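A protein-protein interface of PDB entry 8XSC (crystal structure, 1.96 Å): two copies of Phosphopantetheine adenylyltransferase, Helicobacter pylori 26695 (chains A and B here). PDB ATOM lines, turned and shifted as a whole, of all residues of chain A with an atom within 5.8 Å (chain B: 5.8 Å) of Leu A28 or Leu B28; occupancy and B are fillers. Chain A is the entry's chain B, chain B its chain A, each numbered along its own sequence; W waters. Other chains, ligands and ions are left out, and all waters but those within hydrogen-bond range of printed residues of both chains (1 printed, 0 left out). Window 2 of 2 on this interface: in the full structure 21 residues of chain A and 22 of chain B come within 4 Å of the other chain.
Met A1 touches Arg B24, but with the chains exchanged Arg A24 does not touch Met B1 (4.3 Å).
Leu A28 touches its own counterpart, Leu B28.
Leu A116 touches Leu B28, but with the chains exchanged Leu A28 does not touch Leu B116 (4.1 Å).
Leu B116 touches its own counterpart, Leu A116.
Positions printed for both chains: 1, 2, 24, 25, 26, 27, 28, 29, 30, 116 and 118.
Of the printed residues of chain B, Met A1 touches Arg B24 and Glu B27.
Of the printed residues of chain B, Leu A28 touches Leu B28 (3.1 Å).
Of the printed residues of chain A, Arg B24 touches Met A1.
Of chain A, only Leu A28 (3.1 Å) and Leu A116 (3.9 Å) come within 4 Å of Leu B28.
Printed residues of chain A within 4 Å of Leu B116: Leu A116 and Phe A118.
The nearest residue of chain B that does not touch Leu A28 is Leu B116 (4.1 Å).
The nearest printed residue of chain A that does not touch Leu B116 is Leu A28 (4.1 Å).
The backbone carbonyl oxygen (O) of Arg B24 sits close to the side-chain sulfur (SD) of Met A1, at 3.4 Å.
The side-chain carboxylate of Glu B27 lies close to the side-chain sulfur of Met A1, 3.4 Å away.
The side-chain carboxylate (OE2) of Glu A27 lies close to the side-chain sulfur (SD) of Met B1.
Leu B28 touches Leu A28 (CD2 to CD2, 3.1 Å).
Leu B28 touches Leu A116.
Leu B116 touches Leu A116.
Leu A116 touches Phe B118 (CD1 to CZ, 3.3 Å).
CZ of Phe A118 touches CD1 of Leu B116, at 3.7 Å.
Hydrophobic or aromatic side chains of chain A that line the printed part of chain B: Met A1, Leu A28, Leu A116 and Phe A118.
Along chain A the printed residues that touch a printed residue of chain B span positions 1 to 118.
Hydrophobic or aromatic side chains of chain B that line the printed part of chain A: Met B1, Leu B28, Leu B116 and Phe B118.
Among the printed residues, 8 pairs touch across the chains.
Water W1 lies within hydrogen-bond range of SD of Met B1 (2.9 Å) and OE2 of Glu A27 (3.1 Å).
The backbone carbonyl oxygen (O) of Leu A28 is in hydrogen-bond range of the side-chain amide nitrogen (NE2) of Gln A2 (2.7 Å).
OE1 of Glu A27 sits at hydrogen-bond distance from NE2 of His A23.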
ATOM      1  N   MET A   1      20.929   1.667  -4.289  1.00  0.00           N
ATOM      2  CA  MET A   1      19.652   1.443  -3.504  1.00  0.00           C
ATOM      3  C   MET A   1      18.469   2.151  -4.191  1.00  0.00           C
ATOM      4  O   MET A   1      17.452   1.493  -4.452  1.00  0.00           O
ATOM      5  CB  MET A   1      19.798   1.969  -2.071  1.00  0.00           C
ATOM      6  CG  MET A   1      18.719   1.476  -1.116  1.00  0.00           C
ATOM      7  SD  MET A   1      18.852   2.173   0.573  1.00  0.00           S
ATOM      8  CE  MET A   1      18.156   0.835   1.547  1.00  0.00           C
ATOM      9  N   GLN A   2      18.617   3.446  -4.476  1.00  0.00           N
ATOM     10  CA  GLN A   2      17.573   4.348  -5.049  1.00  0.00           C
ATOM     11  C   GLN A   2      17.334   4.118  -6.554  1.00  0.00           C
ATOM     12  O   GLN A   2      16.407   4.757  -7.092  1.00  0.00           O
ATOM     13  CB  GLN A   2      17.986   5.798  -4.774  1.00  0.00           C
ATOM     14  CG  GLN A   2      16.890   6.816  -5.047  1.00  0.00           C
ATOM     15  CD  GLN A   2      17.034   7.447  -6.415  1.00  0.00           C
ATOM     16  OE1 GLN A   2      18.110   7.401  -7.027  1.00  0.00           O
ATOM     17  NE2 GLN A   2      15.945   8.020  -6.912  1.00  0.00           N
ATOM     18  N   HIS A  23       2.448   5.877  -6.277  1.00  0.00           N
ATOM     19  CA  HIS A  23       2.713   7.331  -6.468  1.00  0.00           C
ATOM     20  C   HIS A  23       3.962   7.731  -5.661  1.00  0.00           C
ATOM     21  O   HIS A  23       4.905   8.338  -6.225  1.00  0.00           O
ATOM     22  CB  HIS A  23       1.508   8.177  -6.012  1.00  0.00           C
ATOM     23  CG  HIS A  23       1.710   9.649  -6.137  1.00  0.00           C
ATOM     24  ND1 HIS A  23       2.242  10.233  -7.292  1.00  0.00           N
ATOM     25  CD2 HIS A  23       1.489  10.666  -5.270  1.00  0.00           C
ATOM     26  CE1 HIS A  23       2.315  11.542  -7.134  1.00  0.00           C
ATOM     27  NE2 HIS A  23       1.847  11.835  -5.904  1.00  0.00           N
ATOM     28  N   ARG A  24       3.957   7.412  -4.373  1.00  0.00           N
ATOM     29  CA  ARG A  24       4.974   7.899  -3.400  1.00  0.00           C
ATOM     30  C   ARG A  24       6.284   7.163  -3.665  1.00  0.00           C
ATOM     31  O   ARG A  24       7.361   7.817  -3.732  1.00  0.00           O
ATOM     32  CB  ARG A  24       4.431   7.667  -1.995  1.00  0.00           C
ATOM     33  CG  ARG A  24       3.230   8.539  -1.701  1.00  0.00           C
ATOM     34  CD  ARG A  24       2.714   8.268  -0.311  1.00  0.00           C
ATOM     35  NE  ARG A  24       1.978   9.433   0.150  1.00  0.00           N
ATOM     36  CZ  ARG A  24       1.341   9.519   1.307  1.00  0.00           C
ATOM     37  NH1 ARG A  24       0.726  10.645   1.609  1.00  0.00           N
ATOM     38  NH2 ARG A  24       1.345   8.505   2.159  1.00  0.00           N
ATOM     39  N   SER A  25       6.181   5.857  -3.915  1.00  0.00           N
ATOM     40  CA  SER A  25       7.348   5.004  -4.183  1.00  0.00           C
ATOM     41  C   SER A  25       7.995   5.388  -5.530  1.00  0.00           C
ATOM     42  O   SER A  25       9.246   5.446  -5.573  1.00  0.00           O
ATOM     43  CB  SER A  25       7.001   3.539  -4.029  1.00  0.00           C
ATOM     44  OG  SER A  25       6.212   3.058  -5.084  1.00  0.00           O
ATOM     45  N   SER A  26       7.221   5.674  -6.577  1.00  0.00           N
ATOM     46  CA  SER A  26       7.778   6.029  -7.914  1.00  0.00           C
ATOM     47  C   SER A  26       8.558   7.356  -7.852  1.00  0.00           C
ATOM     48  O   SER A  26       9.435   7.531  -8.699  1.00  0.00           O
ATOM     49  CB  SER A  26       6.738   6.089  -8.996  1.00  0.00           C
ATOM     50  OG  SER A  26       5.681   6.951  -8.661  1.00  0.00           O
ATOM     51  N   GLU A  27       8.252   8.231  -6.882  1.00  0.00           N
ATOM     52  CA  GLU A  27       8.908   9.550  -6.663  1.00  0.00           C
ATOM     53  C   GLU A  27      10.297   9.355  -6.070  1.00  0.00           C
ATOM     54  O   GLU A  27      11.144  10.245  -6.227  1.00  0.00           O
ATOM     55  CB  GLU A  27       8.119  10.413  -5.682  1.00  0.00           C
ATOM     56  CG  GLU A  27       6.945  11.141  -6.310  1.00  0.00           C
ATOM     57  CD  GLU A  27       6.220  12.045  -5.325  1.00  0.00           C
ATOM     58  OE1 GLU A  27       5.058  11.743  -4.982  1.00  0.00           O
ATOM     59  OE2 GLU A  27       6.836  13.045  -4.883  1.00  0.00           O
ATOM     60  N   LEU A  28      10.516   8.244  -5.376  1.00  0.00           N
ATOM     61  CA  LEU A  28      11.759   8.003  -4.606  1.00  0.00           C
ATOM     62  C   LEU A  28      12.779   7.193  -5.411  1.00  0.00           C
ATOM     63  O   LEU A  28      13.992   7.353  -5.141  1.00  0.00           O
ATOM     64  CB  LEU A  28      11.350   7.273  -3.331  1.00  0.00           C
ATOM     65  CG  LEU A  28      12.495   6.945  -2.394  1.00  0.00           C
ATOM     66  CD1 LEU A  28      13.154   8.221  -1.874  1.00  0.00           C
ATOM     67  CD2 LEU A  28      11.989   6.068  -1.255  1.00  0.00           C
ATOM     68  N   PHE A  29      12.313   6.359  -6.339  1.00  0.00           N
ATOM     69  CA  PHE A  29      13.121   5.383  -7.112  1.00  0.00           C
ATOM     70  C   PHE A  29      13.196   5.809  -8.572  1.00  0.00           C
ATOM     71  O   PHE A  29      12.213   6.267  -9.110  1.00  0.00           O
ATOM     72  CB  PHE A  29      12.538   3.971  -7.018  1.00  0.00           C
ATOM     73  CG  PHE A  29      12.641   3.409  -5.632  1.00  0.00           C
ATOM     74  CD1 PHE A  29      13.864   2.992  -5.142  1.00  0.00           C
ATOM     75  CD2 PHE A  29      11.532   3.353  -4.798  1.00  0.00           C
ATOM     76  CE1 PHE A  29      13.978   2.494  -3.855  1.00  0.00           C
ATOM     77  CE2 PHE A  29      11.646   2.836  -3.516  1.00  0.00           C
ATOM     78  CZ  PHE A  29      12.875   2.450  -3.029  1.00  0.00           C
ATOM     79  N   GLU A  30      14.353   5.635  -9.198  1.00  0.00           N
ATOM     80  CA  GLU A  30      14.499   6.027 -10.617  1.00  0.00           C
ATOM     81  C   GLU A  30      13.535   5.154 -11.430  1.00  0.00           C
ATOM     82  O   GLU A  30      13.090   5.623 -12.484  1.00  0.00           O
ATOM     83  CB  GLU A  30      15.967   5.970 -11.039  1.00  0.00           C
ATOM     84  CG  GLU A  30      16.778   7.143 -10.502  1.00  0.00           C
ATOM     85  CD  GLU A  30      18.277   7.148 -10.821  1.00  0.00           C
ATOM     86  OE1 GLU A  30      18.705   6.392 -11.723  1.00  0.00           O
ATOM     87  OE2 GLU A  30      19.028   7.947 -10.180  1.00  0.00           O
ATOM     88  N   LEU A 116      10.878  -1.621   2.534  1.00  0.00           N
ATOM     89  CA  LEU A 116      10.508  -0.230   2.862  1.00  0.00           C
ATOM     90  C   LEU A 116       8.981  -0.140   2.888  1.00  0.00           C
ATOM     91  O   LEU A 116       8.321  -0.615   1.921  1.00  0.00           O
ATOM     92  CB  LEU A 116      11.147   0.618   1.761  1.00  0.00           C
ATOM     93  CG  LEU A 116      11.083   2.124   1.906  1.00  0.00           C
ATOM     94  CD1 LEU A 116      11.525   2.541   3.298  1.00  0.00           C
ATOM     95  CD2 LEU A 116      11.946   2.782   0.827  1.00  0.00           C
ATOM     96  N   PHE A 118       5.472   2.113   2.896  1.00  0.00           N
ATOM     97  CA  PHE A 118       4.738   3.366   2.589  1.00  0.00           C
ATOM     98  C   PHE A 118       3.320   3.275   3.170  1.00  0.00           C
ATOM     99  O   PHE A 118       2.810   2.150   3.492  1.00  0.00           O
ATOM    100  CB  PHE A 118       4.752   3.662   1.086  1.00  0.00           C
ATOM    101  CG  PHE A 118       6.113   3.916   0.491  1.00  0.00           C
ATOM    102  CD1 PHE A 118       7.006   2.867   0.290  1.00  0.00           C
ATOM    103  CD2 PHE A 118       6.496   5.190   0.093  1.00  0.00           C
ATOM    104  CE1 PHE A 118       8.248   3.084  -0.285  1.00  0.00           C
ATOM    105  CE2 PHE A 118       7.746   5.406  -0.464  1.00  0.00           C
ATOM    106  CZ  PHE A 118       8.620   4.355  -0.644  1.00  0.00           C
ATOM    107  N   MET B   1      11.585  15.160  -3.107  1.00  0.00           N
ATOM    108  CA  MET B   1      11.316  14.074  -2.094  1.00  0.00           C
ATOM    109  C   MET B   1      12.651  13.432  -1.692  1.00  0.00           C
ATOM    110  O   MET B   1      12.888  13.310  -0.477  1.00  0.00           O
ATOM    111  CB  MET B   1      10.351  13.006  -2.643  1.00  0.00           C
ATOM    112  CG  MET B   1       9.413  12.393  -1.586  1.00  0.00           C
ATOM    113  SD  MET B   1       7.774  11.825  -2.199  1.00  0.00           S
ATOM    114  CE  MET B   1       7.012  11.236  -0.687  1.00  0.00           C
ATOM    115  N   GLN B   2      13.500  13.108  -2.679  1.00  0.00           N
ATOM    116  CA  GLN B   2      14.824  12.448  -2.523  1.00  0.00           C
ATOM    117  C   GLN B   2      15.914  13.424  -2.050  1.00  0.00           C
ATOM    118  O   GLN B   2      16.991  12.938  -1.712  1.00  0.00           O
ATOM    119  CB  GLN B   2      15.268  11.814  -3.844  1.00  0.00           C
ATOM    120  CG  GLN B   2      16.378  10.779  -3.684  1.00  0.00           C
ATOM    121  CD  GLN B   2      17.683  11.175  -4.336  1.00  0.00           C
ATOM    122  OE1 GLN B   2      17.696  11.811  -5.387  1.00  0.00           O
ATOM    123  NE2 GLN B   2      18.795  10.786  -3.725  1.00  0.00           N
ATOM    124  N   ARG B  24      20.384   2.799   6.587  1.00  0.00           N
ATOM    125  CA  ARG B  24      19.553   2.388   5.427  1.00  0.00           C
ATOM    126  C   ARG B  24      18.863   3.611   4.831  1.00  0.00           C
ATOM    127  O   ARG B  24      18.811   3.737   3.582  1.00  0.00           O
ATOM    128  CB  ARG B  24      18.514   1.359   5.883  1.00  0.00           C
ATOM    129  CG  ARG B  24      19.120  -0.026   6.073  1.00  0.00           C
ATOM    130  CD  ARG B  24      18.270  -0.970   6.913  1.00  0.00           C
ATOM    131  NE  ARG B  24      18.946  -2.262   7.042  1.00  0.00           N
ATOM    132  CZ  ARG B  24      18.380  -3.405   7.441  1.00  0.00           C
ATOM    133  NH1 ARG B  24      19.112  -4.511   7.501  1.00  0.00           N
ATOM    134  NH2 ARG B  24      17.095  -3.450   7.754  1.00  0.00           N
ATOM    135  N   SER B  25      18.291   4.453   5.682  1.00  0.00           N
ATOM    136  CA  SER B  25      17.520   5.640   5.213  1.00  0.00           C
ATOM    137  C   SER B  25      18.460   6.673   4.569  1.00  0.00           C
ATOM    138  O   SER B  25      18.078   7.217   3.508  1.00  0.00           O
ATOM    139  CB  SER B  25      16.728   6.242   6.317  1.00  0.00           C
ATOM    140  OG  SER B  25      17.600   6.790   7.268  1.00  0.00           O
ATOM    141  N   SER B  26      19.654   6.892   5.129  1.00  0.00           N
ATOM    142  CA  SER B  26      20.686   7.794   4.542  1.00  0.00           C
ATOM    143  C   SER B  26      21.091   7.361   3.122  1.00  0.00           C
ATOM    144  O   SER B  26      21.449   8.242   2.348  1.00  0.00           O
ATOM    145  CB  SER B  26      21.887   7.980   5.425  1.00  0.00           C
ATOM    146  OG  SER B  26      22.741   6.848   5.436  1.00  0.00           O
ATOM    147  N   GLU B  27      21.039   6.080   2.775  1.00  0.00           N
ATOM    148  CA  GLU B  27      21.396   5.611   1.409  1.00  0.00           C
ATOM    149  C   GLU B  27      20.309   6.060   0.421  1.00  0.00           C
ATOM    150  O   GLU B  27      20.555   6.033  -0.764  1.00  0.00           O
ATOM    151  CB  GLU B  27      21.558   4.092   1.377  1.00  0.00           C
ATOM    152  CG  GLU B  27      22.769   3.591   2.150  1.00  0.00           C
ATOM    153  CD  GLU B  27      22.821   2.084   2.349  1.00  0.00           C
ATOM    154  OE1 GLU B  27      23.819   1.600   2.916  1.00  0.00           O
ATOM    155  OE2 GLU B  27      21.849   1.386   1.968  1.00  0.00           O
ATOM    156  N   LEU B  28      19.123   6.438   0.889  1.00  0.00           N
ATOM    157  CA  LEU B  28      17.989   6.705  -0.034  1.00  0.00           C
ATOM    158  C   LEU B  28      17.825   8.213  -0.296  1.00  0.00           C
ATOM    159  O   LEU B  28      17.297   8.565  -1.345  1.00  0.00           O
ATOM    160  CB  LEU B  28      16.763   6.050   0.604  1.00  0.00           C
ATOM    161  CG  LEU B  28      15.442   6.299  -0.097  1.00  0.00           C
ATOM    162  CD1 LEU B  28      15.433   5.612  -1.462  1.00  0.00           C
ATOM    163  CD2 LEU B  28      14.312   5.827   0.809  1.00  0.00           C
ATOM    164  N   PHE B  29      18.249   9.080   0.630  1.00  0.00           N
ATOM    165  CA  PHE B  29      18.120  10.558   0.545  1.00  0.00           C
ATOM    166  C   PHE B  29      19.503  11.180   0.303  1.00  0.00           C
ATOM    167  O   PHE B  29      20.457  10.636   0.844  1.00  0.00           O
ATOM    168  CB  PHE B  29      17.531  11.117   1.843  1.00  0.00           C
ATOM    169  CG  PHE B  29      16.158  10.590   2.094  1.00  0.00           C
ATOM    170  CD1 PHE B  29      15.070  11.138   1.431  1.00  0.00           C
ATOM    171  CD2 PHE B  29      15.975   9.437   2.845  1.00  0.00           C
ATOM    172  CE1 PHE B  29      13.807  10.594   1.584  1.00  0.00           C
ATOM    173  CE2 PHE B  29      14.708   8.898   2.991  1.00  0.00           C
ATOM    174  CZ  PHE B  29      13.626   9.486   2.380  1.00  0.00           C
ATOM    175  N   GLU B  30      19.596  12.297  -0.428  1.00  0.00           N
ATOM    176  CA  GLU B  30      20.880  13.025  -0.626  1.00  0.00           C
ATOM    177  C   GLU B  30      21.405  13.506   0.736  1.00  0.00           C
ATOM    178  O   GLU B  30      22.613  13.517   0.916  1.00  0.00           O
ATOM    179  CB  GLU B  30      20.728  14.196  -1.596  1.00  0.00           C
ATOM    180  CG  GLU B  30      20.676  13.787  -3.061  1.00  0.00           C
ATOM    181  CD  GLU B  30      20.493  14.973  -3.994  1.00  0.00           C
ATOM    182  OE1 GLU B  30      20.423  16.117  -3.490  1.00  0.00           O
ATOM    183  OE2 GLU B  30      20.411  14.772  -5.223  1.00  0.00           O
ATOM    184  N   LEU B 116       7.624   7.398   5.904  1.00  0.00           N
ATOM    185  CA  LEU B 116       8.185   6.184   5.294  1.00  0.00           C
ATOM    186  C   LEU B 116       8.759   5.325   6.434  1.00  0.00           C
ATOM    187  O   LEU B 116       9.309   5.925   7.349  1.00  0.00           O
ATOM    188  CB  LEU B 116       9.236   6.707   4.314  1.00  0.00           C
ATOM    189  CG  LEU B 116      10.101   5.646   3.674  1.00  0.00           C
ATOM    190  CD1 LEU B 116       9.212   4.620   2.977  1.00  0.00           C
ATOM    191  CD2 LEU B 116      11.047   6.277   2.682  1.00  0.00           C
ATOM    192  N   PHE B 118      11.315   2.078   7.731  1.00  0.00           N
ATOM    193  CA  PHE B 118      12.401   1.107   7.534  1.00  0.00           C
ATOM    194  C   PHE B 118      12.377   0.135   8.698  1.00  0.00           C
ATOM    195  O   PHE B 118      11.680   0.381   9.736  1.00  0.00           O
ATOM    196  CB  PHE B 118      13.757   1.805   7.449  1.00  0.00           C
ATOM    197  CG  PHE B 118      13.897   2.717   6.258  1.00  0.00           C
ATOM    198  CD1 PHE B 118      13.259   3.950   6.234  1.00  0.00           C
ATOM    199  CD2 PHE B 118      14.678   2.364   5.170  1.00  0.00           C
ATOM    200  CE1 PHE B 118      13.395   4.813   5.155  1.00  0.00           C
ATOM    201  CE2 PHE B 118      14.806   3.228   4.089  1.00  0.00           C
ATOM    202  CZ  PHE B 118      14.152   4.436   4.077  1.00  0.00           C
HETATM  203  O   HOH W   1       7.954  14.683  -2.452  1.00  0.00           O
